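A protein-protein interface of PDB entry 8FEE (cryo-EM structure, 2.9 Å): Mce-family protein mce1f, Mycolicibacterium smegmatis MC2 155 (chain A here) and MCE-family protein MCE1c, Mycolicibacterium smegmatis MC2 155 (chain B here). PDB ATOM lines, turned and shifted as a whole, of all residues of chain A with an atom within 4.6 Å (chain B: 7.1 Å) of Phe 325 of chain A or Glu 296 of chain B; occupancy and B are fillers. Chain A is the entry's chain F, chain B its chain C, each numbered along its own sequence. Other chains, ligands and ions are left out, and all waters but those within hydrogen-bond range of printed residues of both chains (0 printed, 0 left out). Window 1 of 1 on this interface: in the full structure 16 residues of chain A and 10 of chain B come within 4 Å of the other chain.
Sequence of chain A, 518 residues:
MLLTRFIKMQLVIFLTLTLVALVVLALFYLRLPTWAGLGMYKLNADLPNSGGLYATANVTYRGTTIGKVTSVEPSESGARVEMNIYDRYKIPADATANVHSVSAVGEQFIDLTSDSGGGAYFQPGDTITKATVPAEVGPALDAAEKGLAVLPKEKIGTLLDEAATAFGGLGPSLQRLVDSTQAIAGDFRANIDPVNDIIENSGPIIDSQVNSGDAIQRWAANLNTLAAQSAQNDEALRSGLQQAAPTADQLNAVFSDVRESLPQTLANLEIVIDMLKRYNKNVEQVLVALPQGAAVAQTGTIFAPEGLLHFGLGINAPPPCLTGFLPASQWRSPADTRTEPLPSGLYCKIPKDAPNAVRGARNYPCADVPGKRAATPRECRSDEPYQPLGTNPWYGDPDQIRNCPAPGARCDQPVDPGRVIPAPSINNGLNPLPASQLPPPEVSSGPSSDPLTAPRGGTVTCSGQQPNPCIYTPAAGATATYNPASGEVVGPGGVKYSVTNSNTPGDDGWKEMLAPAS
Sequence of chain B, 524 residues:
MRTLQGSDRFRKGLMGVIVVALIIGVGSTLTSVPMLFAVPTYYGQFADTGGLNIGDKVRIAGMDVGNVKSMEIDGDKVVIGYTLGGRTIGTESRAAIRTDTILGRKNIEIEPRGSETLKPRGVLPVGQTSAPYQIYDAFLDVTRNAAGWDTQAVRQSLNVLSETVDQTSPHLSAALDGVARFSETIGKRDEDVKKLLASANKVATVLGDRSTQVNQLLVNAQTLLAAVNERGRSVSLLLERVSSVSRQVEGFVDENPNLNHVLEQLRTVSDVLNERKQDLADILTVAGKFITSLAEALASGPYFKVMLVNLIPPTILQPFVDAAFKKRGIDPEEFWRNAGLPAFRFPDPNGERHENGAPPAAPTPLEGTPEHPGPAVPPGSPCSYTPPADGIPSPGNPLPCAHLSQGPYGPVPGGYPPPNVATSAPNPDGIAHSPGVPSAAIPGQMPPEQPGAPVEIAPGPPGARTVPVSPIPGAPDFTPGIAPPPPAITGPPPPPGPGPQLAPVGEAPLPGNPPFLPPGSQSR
Of the printed residues of chain B, Phe 325 of chain A touches Glu 296. Glu 296 of chain B touches five residues of chain A. No residue of chain B comes within 4 Å of Gly 324 of chain A. Of the printed residues of chain B, Ala 361 of chain A touches Glu 296. Printed residues of chain B within 4 Å of Cys 348 of chain A: Glu 296 (3.2 Å). Of the printed residues of chain B, Tyr 347 of chain A touches Glu 296. Of the printed residues of chain B, Gly 360 of chain A touches Glu 296 (3.6 Å) and Ala 299 (3.7 Å). Of the printed residues of chain A, Ser 293 of chain B touches Leu 346 (3.5 Å). Leu 326 of chain A touches none of the printed residues of chain B. The nearest printed residue of chain A that does not touch Glu 296 of chain B is Cys 321 of chain A (5.5 Å).
The backbone NH (N) of Cys 348 of chain A sits close to the side-chain carboxylate (OE2) of Glu 296 of chain B (3.4 Å). The side-chain carboxylate (OE1) of Glu 296 of chain B sits at hydrogen-bond distance from the backbone NH (N) of Ala 361 of chain A, at 2.9 Å.
Among the printed residues, 7 pairs touch across the chains. Among the printed residues, no Asp or Glu carboxylate lies within 4 Å of a Lys or Arg side-chain nitrogen of the other chain.
Phe 325 of chain A touches Glu 296 of chain B (CZ to CG, 3.8 Å). Ser 293 of chain B touches Leu 346 of chain A (CB to O, 3.5 Å). Tyr 347 of chain A touches Glu 296 of chain B. Gly 360 of chain A touches Glu 296 of chain B (CA to OE2, 3.6 Å). N of Gly 360 of chain A touches CB of Ala 299 of chain B, at 3.7 Å.
N of Tyr 347 of chain A is in hydrogen-bond range of O of Gly 324 of chain A, at 3.4 Å. The side-chain sulfur of Cys 321 of chain A forms a disulfide with the side-chain sulfur of Cys 348 of chain A.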
ATOM      1  N   CYS A 321      -3.026 -11.071   2.881  1.00  0.00           N
ATOM      2  CA  CYS A 321      -1.816 -10.610   3.543  1.00  0.00           C
ATOM      3  C   CYS A 321      -0.690 -11.621   3.368  1.00  0.00           C
ATOM      4  O   CYS A 321      -0.903 -12.833   3.457  1.00  0.00           O
ATOM      5  CB  CYS A 321      -2.098 -10.325   5.021  1.00  0.00           C
ATOM      6  SG  CYS A 321      -2.841 -11.699   5.910  1.00  0.00           S
ATOM      7  N   LEU A 322       0.512 -11.105   3.115  1.00  0.00           N
ATOM      8  CA  LEU A 322       1.728 -11.904   3.044  1.00  0.00           C
ATOM      9  C   LEU A 322       2.646 -11.697   4.242  1.00  0.00           C
ATOM     10  O   LEU A 322       3.793 -12.154   4.216  1.00  0.00           O
ATOM     11  CB  LEU A 322       2.481 -11.599   1.747  1.00  0.00           C
ATOM     12  CG  LEU A 322       1.681 -11.738   0.450  1.00  0.00           C
ATOM     13  CD1 LEU A 322       2.567 -11.474  -0.757  1.00  0.00           C
ATOM     14  CD2 LEU A 322       1.042 -13.112   0.355  1.00  0.00           C
ATOM     15  N   THR A 323       2.176 -11.020   5.287  1.00  0.00           N
ATOM     16  CA  THR A 323       2.985 -10.769   6.471  1.00  0.00           C
ATOM     17  C   THR A 323       2.799 -11.903   7.468  1.00  0.00           C
ATOM     18  O   THR A 323       1.668 -12.266   7.805  1.00  0.00           O
ATOM     19  CB  THR A 323       2.607  -9.437   7.119  1.00  0.00           C
ATOM     20  OG1 THR A 323       1.234  -9.477   7.527  1.00  0.00           O
ATOM     21  CG2 THR A 323       2.807  -8.297   6.142  1.00  0.00           C
ATOM     22  N   GLY A 324       3.914 -12.452   7.945  1.00  0.00           N
ATOM     23  CA  GLY A 324       3.882 -13.592   8.831  1.00  0.00           C
ATOM     24  C   GLY A 324       3.769 -14.932   8.145  1.00  0.00           C
ATOM     25  O   GLY A 324       3.640 -15.953   8.835  1.00  0.00           O
ATOM     26  N   PHE A 325       3.809 -14.969   6.819  1.00  0.00           N
ATOM     27  CA  PHE A 325       3.757 -16.202   6.051  1.00  0.00           C
ATOM     28  C   PHE A 325       5.077 -16.401   5.317  1.00  0.00           C
ATOM     29  O   PHE A 325       6.011 -15.602   5.437  1.00  0.00           O
ATOM     30  CB  PHE A 325       2.579 -16.179   5.077  1.00  0.00           C
ATOM     31  CG  PHE A 325       1.242 -16.298   5.742  1.00  0.00           C
ATOM     32  CD1 PHE A 325       0.847 -17.489   6.325  1.00  0.00           C
ATOM     33  CD2 PHE A 325       0.375 -15.222   5.776  1.00  0.00           C
ATOM     34  CE1 PHE A 325      -0.387 -17.601   6.935  1.00  0.00           C
ATOM     35  CE2 PHE A 325      -0.859 -15.329   6.385  1.00  0.00           C
ATOM     36  CZ  PHE A 325      -1.241 -16.519   6.964  1.00  0.00           C
ATOM     37  N   LEU A 326       5.148 -17.487   4.556  1.00  0.00           N
ATOM     38  CA  LEU A 326       6.375 -17.830   3.853  1.00  0.00           C
ATOM     39  C   LEU A 326       6.685 -16.779   2.788  1.00  0.00           C
ATOM     40  O   LEU A 326       5.773 -16.305   2.102  1.00  0.00           O
ATOM     41  CB  LEU A 326       6.246 -19.210   3.210  1.00  0.00           C
ATOM     42  CG  LEU A 326       7.513 -19.918   2.736  1.00  0.00           C
ATOM     43  CD1 LEU A 326       8.400 -20.272   3.916  1.00  0.00           C
ATOM     44  CD2 LEU A 326       7.159 -21.161   1.939  1.00  0.00           C
ATOM     45  N   PRO A 327       7.949 -16.383   2.639  1.00  0.00           N
ATOM     46  CA  PRO A 327       8.299 -15.408   1.599  1.00  0.00           C
ATOM     47  C   PRO A 327       8.048 -15.968   0.208  1.00  0.00           C
ATOM     48  O   PRO A 327       8.073 -17.180  -0.010  1.00  0.00           O
ATOM     49  CB  PRO A 327       9.790 -15.150   1.838  1.00  0.00           C
ATOM     50  CG  PRO A 327      10.026 -15.555   3.253  1.00  0.00           C
ATOM     51  CD  PRO A 327       9.094 -16.695   3.508  1.00  0.00           C
ATOM     52  N   LEU A 346       2.917 -19.685  11.743  1.00  0.00           N
ATOM     53  CA  LEU A 346       2.579 -19.001  10.500  1.00  0.00           C
ATOM     54  C   LEU A 346       1.146 -18.495  10.584  1.00  0.00           C
ATOM     55  O   LEU A 346       0.204 -19.293  10.636  1.00  0.00           O
ATOM     56  CB  LEU A 346       2.754 -19.926   9.297  1.00  0.00           C
ATOM     57  CG  LEU A 346       4.187 -20.299   8.924  1.00  0.00           C
ATOM     58  CD1 LEU A 346       4.201 -21.156   7.671  1.00  0.00           C
ATOM     59  CD2 LEU A 346       5.029 -19.048   8.731  1.00  0.00           C
ATOM     60  N   TYR A 347       0.987 -17.174  10.587  1.00  0.00           N
ATOM     61  CA  TYR A 347      -0.325 -16.551  10.474  1.00  0.00           C
ATOM     62  C   TYR A 347      -0.131 -15.099  10.060  1.00  0.00           C
ATOM     63  O   TYR A 347       0.979 -14.563  10.084  1.00  0.00           O
ATOM     64  CB  TYR A 347      -1.128 -16.662  11.777  1.00  0.00           C
ATOM     65  CG  TYR A 347      -0.458 -16.072  12.998  1.00  0.00           C
ATOM     66  CD1 TYR A 347       0.422 -16.824  13.765  1.00  0.00           C
ATOM     67  CD2 TYR A 347      -0.724 -14.769  13.396  1.00  0.00           C
ATOM     68  CE1 TYR A 347       1.030 -16.290  14.884  1.00  0.00           C
ATOM     69  CE2 TYR A 347      -0.120 -14.228  14.512  1.00  0.00           C
ATOM     70  CZ  TYR A 347       0.753 -14.992  15.253  1.00  0.00           C
ATOM     71  OH  TYR A 347       1.353 -14.451  16.366  1.00  0.00           O
ATOM     72  N   CYS A 348      -1.238 -14.478   9.659  1.00  0.00           N
ATOM     73  CA  CYS A 348      -1.228 -13.094   9.202  1.00  0.00           C
ATOM     74  C   CYS A 348      -0.828 -12.152  10.334  1.00  0.00           C
ATOM     75  O   CYS A 348      -1.366 -12.231  11.443  1.00  0.00           O
ATOM     76  CB  CYS A 348      -2.610 -12.749   8.658  1.00  0.00           C
ATOM     77  SG  CYS A 348      -2.852 -11.159   7.870  1.00  0.00           S
ATOM     78  N   GLY A 360      -8.884 -13.526  11.883  1.00  0.00           N
ATOM     79  CA  GLY A 360      -7.731 -14.394  11.762  1.00  0.00           C
ATOM     80  C   GLY A 360      -7.258 -14.968  13.082  1.00  0.00           C
ATOM     81  O   GLY A 360      -7.996 -14.975  14.069  1.00  0.00           O
ATOM     82  N   ALA A 361      -6.014 -15.448  13.107  1.00  0.00           N
ATOM     83  CA  ALA A 361      -5.485 -16.083  14.310  1.00  0.00           C
ATOM     84  C   ALA A 361      -5.355 -15.090  15.458  1.00  0.00           C
ATOM     85  O   ALA A 361      -5.733 -15.394  16.594  1.00  0.00           O
ATOM     86  CB  ALA A 361      -4.138 -16.734  14.007  1.00  0.00           C
ATOM     87  N   PHE B 290      -0.672 -26.743  12.340  1.00  0.00           N
ATOM     88  CA  PHE B 290      -1.194 -26.233  11.072  1.00  0.00           C
ATOM     89  C   PHE B 290      -2.620 -25.708  11.144  1.00  0.00           C
ATOM     90  O   PHE B 290      -3.075 -25.111  10.161  1.00  0.00           O
ATOM     91  CB  PHE B 290      -1.128 -27.299   9.954  1.00  0.00           C
ATOM     92  CG  PHE B 290      -2.294 -28.275   9.927  1.00  0.00           C
ATOM     93  CD1 PHE B 290      -3.433 -28.010   9.172  1.00  0.00           C
ATOM     94  CD2 PHE B 290      -2.227 -29.477  10.596  1.00  0.00           C
ATOM     95  CE1 PHE B 290      -4.486 -28.903   9.137  1.00  0.00           C
ATOM     96  CE2 PHE B 290      -3.277 -30.373  10.561  1.00  0.00           C
ATOM     97  CZ  PHE B 290      -4.406 -30.086   9.830  1.00  0.00           C
ATOM     98  N   ILE B 291      -3.337 -25.910  12.251  1.00  0.00           N
ATOM     99  CA  ILE B 291      -4.744 -25.524  12.295  1.00  0.00           C
ATOM    100  C   ILE B 291      -4.895 -24.006  12.219  1.00  0.00           C
ATOM    101  O   ILE B 291      -5.809 -23.494  11.561  1.00  0.00           O
ATOM    102  CB  ILE B 291      -5.424 -26.115  13.544  1.00  0.00           C
ATOM    103  CG1 ILE B 291      -6.907 -25.763  13.568  1.00  0.00           C
ATOM    104  CG2 ILE B 291      -4.768 -25.623  14.825  1.00  0.00           C
ATOM    105  CD1 ILE B 291      -7.628 -26.375  14.727  1.00  0.00           C
ATOM    106  N   THR B 292      -3.996 -23.264  12.873  1.00  0.00           N
ATOM    107  CA  THR B 292      -4.059 -21.806  12.827  1.00  0.00           C
ATOM    108  C   THR B 292      -3.797 -21.278  11.423  1.00  0.00           C
ATOM    109  O   THR B 292      -4.481 -20.355  10.966  1.00  0.00           O
ATOM    110  CB  THR B 292      -3.064 -21.203  13.818  1.00  0.00           C
ATOM    111  OG1 THR B 292      -1.773 -21.791  13.622  1.00  0.00           O
ATOM    112  CG2 THR B 292      -3.521 -21.454  15.247  1.00  0.00           C
ATOM    113  N   SER B 293      -2.808 -21.841  10.728  1.00  0.00           N
ATOM    114  CA  SER B 293      -2.513 -21.383   9.375  1.00  0.00           C
ATOM    115  C   SER B 293      -3.622 -21.762   8.403  1.00  0.00           C
ATOM    116  O   SER B 293      -3.945 -20.991   7.492  1.00  0.00           O
ATOM    117  CB  SER B 293      -1.176 -21.952   8.905  1.00  0.00           C
ATOM    118  OG  SER B 293      -1.010 -21.752   7.512  1.00  0.00           O
ATOM    119  N   LEU B 294      -4.211 -22.948   8.573  1.00  0.00           N
ATOM    120  CA  LEU B 294      -5.253 -23.386   7.650  1.00  0.00           C
ATOM    121  C   LEU B 294      -6.550 -22.614   7.860  1.00  0.00           C
ATOM    122  O   LEU B 294      -7.195 -22.203   6.889  1.00  0.00           O
ATOM    123  CB  LEU B 294      -5.485 -24.888   7.801  1.00  0.00           C
ATOM    124  CG  LEU B 294      -6.232 -25.568   6.656  1.00  0.00           C
ATOM    125  CD1 LEU B 294      -5.373 -25.596   5.408  1.00  0.00           C
ATOM    126  CD2 LEU B 294      -6.629 -26.974   7.049  1.00  0.00           C
ATOM    127  N   ALA B 295      -6.950 -22.402   9.117  1.00  0.00           N
ATOM    128  CA  ALA B 295      -8.148 -21.622   9.404  1.00  0.00           C
ATOM    129  C   ALA B 295      -7.992 -20.143   9.085  1.00  0.00           C
ATOM    130  O   ALA B 295      -8.990 -19.417   9.109  1.00  0.00           O
ATOM    131  CB  ALA B 295      -8.541 -21.778  10.874  1.00  0.00           C
ATOM    132  N   GLU B 296      -6.771 -19.680   8.803  1.00  0.00           N
ATOM    133  CA  GLU B 296      -6.563 -18.276   8.470  1.00  0.00           C
ATOM    134  C   GLU B 296      -7.283 -17.881   7.187  1.00  0.00           C
ATOM    135  O   GLU B 296      -7.653 -16.715   7.019  1.00  0.00           O
ATOM    136  CB  GLU B 296      -5.067 -17.982   8.352  1.00  0.00           C
ATOM    137  CG  GLU B 296      -4.719 -16.509   8.445  1.00  0.00           C
ATOM    138  CD  GLU B 296      -4.734 -16.001   9.875  1.00  0.00           C
ATOM    139  OE1 GLU B 296      -4.909 -16.822  10.799  1.00  0.00           O
ATOM    140  OE2 GLU B 296      -4.581 -14.781  10.079  1.00  0.00           O
ATOM    141  N   ALA B 297      -7.486 -18.834   6.275  1.00  0.00           N
ATOM    142  CA  ALA B 297      -8.068 -18.517   4.974  1.00  0.00           C
ATOM    143  C   ALA B 297      -9.497 -18.012   5.106  1.00  0.00           C
ATOM    144  O   ALA B 297      -9.878 -17.019   4.475  1.00  0.00           O
ATOM    145  CB  ALA B 297      -8.013 -19.744   4.065  1.00  0.00           C
ATOM    146  N   LEU B 298     -10.302 -18.675   5.926  1.00  0.00           N
ATOM    147  CA  LEU B 298     -11.711 -18.319   6.078  1.00  0.00           C
ATOM    148  C   LEU B 298     -11.906 -17.210   7.109  1.00  0.00           C
ATOM    149  O   LEU B 298     -12.695 -17.337   8.043  1.00  0.00           O
ATOM    150  CB  LEU B 298     -12.514 -19.559   6.454  1.00  0.00           C
ATOM    151  CG  LEU B 298     -11.723 -20.836   6.748  1.00  0.00           C
ATOM    152  CD1 LEU B 298     -12.494 -21.701   7.703  1.00  0.00           C
ATOM    153  CD2 LEU B 298     -11.444 -21.624   5.478  1.00  0.00           C
ATOM    154  N   ALA B 299     -11.190 -16.100   6.937  1.00  0.00           N
ATOM    155  CA  ALA B 299     -11.176 -15.032   7.926  1.00  0.00           C
ATOM    156  C   ALA B 299     -11.578 -13.672   7.381  1.00  0.00           C
ATOM    157  O   ALA B 299     -12.079 -12.848   8.146  1.00  0.00           O
ATOM    158  CB  ALA B 299      -9.786 -14.908   8.568  1.00  0.00           C
ATOM    159  N   SER B 300     -11.352 -13.399   6.097  1.00  0.00           N
ATOM    160  CA  SER B 300     -11.642 -12.077   5.558  1.00  0.00           C
ATOM    161  C   SER B 300     -13.118 -11.866   5.257  1.00  0.00           C
ATOM    162  O   SER B 300     -13.542 -10.719   5.089  1.00  0.00           O
ATOM    163  CB  SER B 300     -10.821 -11.828   4.294  1.00  0.00           C
ATOM    164  OG  SER B 300      -9.434 -11.811   4.583  1.00  0.00           O
ATOM    165  N   LYS B 305     -10.445 -17.920   0.794  1.00  0.00           N
ATOM    166  CA  LYS B 305      -9.621 -17.565  -0.351  1.00  0.00           C
ATOM    167  C   LYS B 305      -9.043 -18.810  -1.009  1.00  0.00           C
ATOM    168  O   LYS B 305      -8.816 -19.836  -0.365  1.00  0.00           O
ATOM    169  CB  LYS B 305      -8.487 -16.631   0.063  1.00  0.00           C
ATOM    170  CG  LYS B 305      -8.947 -15.299   0.607  1.00  0.00           C
ATOM    171  CD  LYS B 305      -7.786 -14.332   0.710  1.00  0.00           C
ATOM    172  CE  LYS B 305      -8.122 -13.200   1.652  1.00  0.00           C
ATOM    173  NZ  LYS B 305      -9.524 -12.764   1.440  1.00  0.00           N
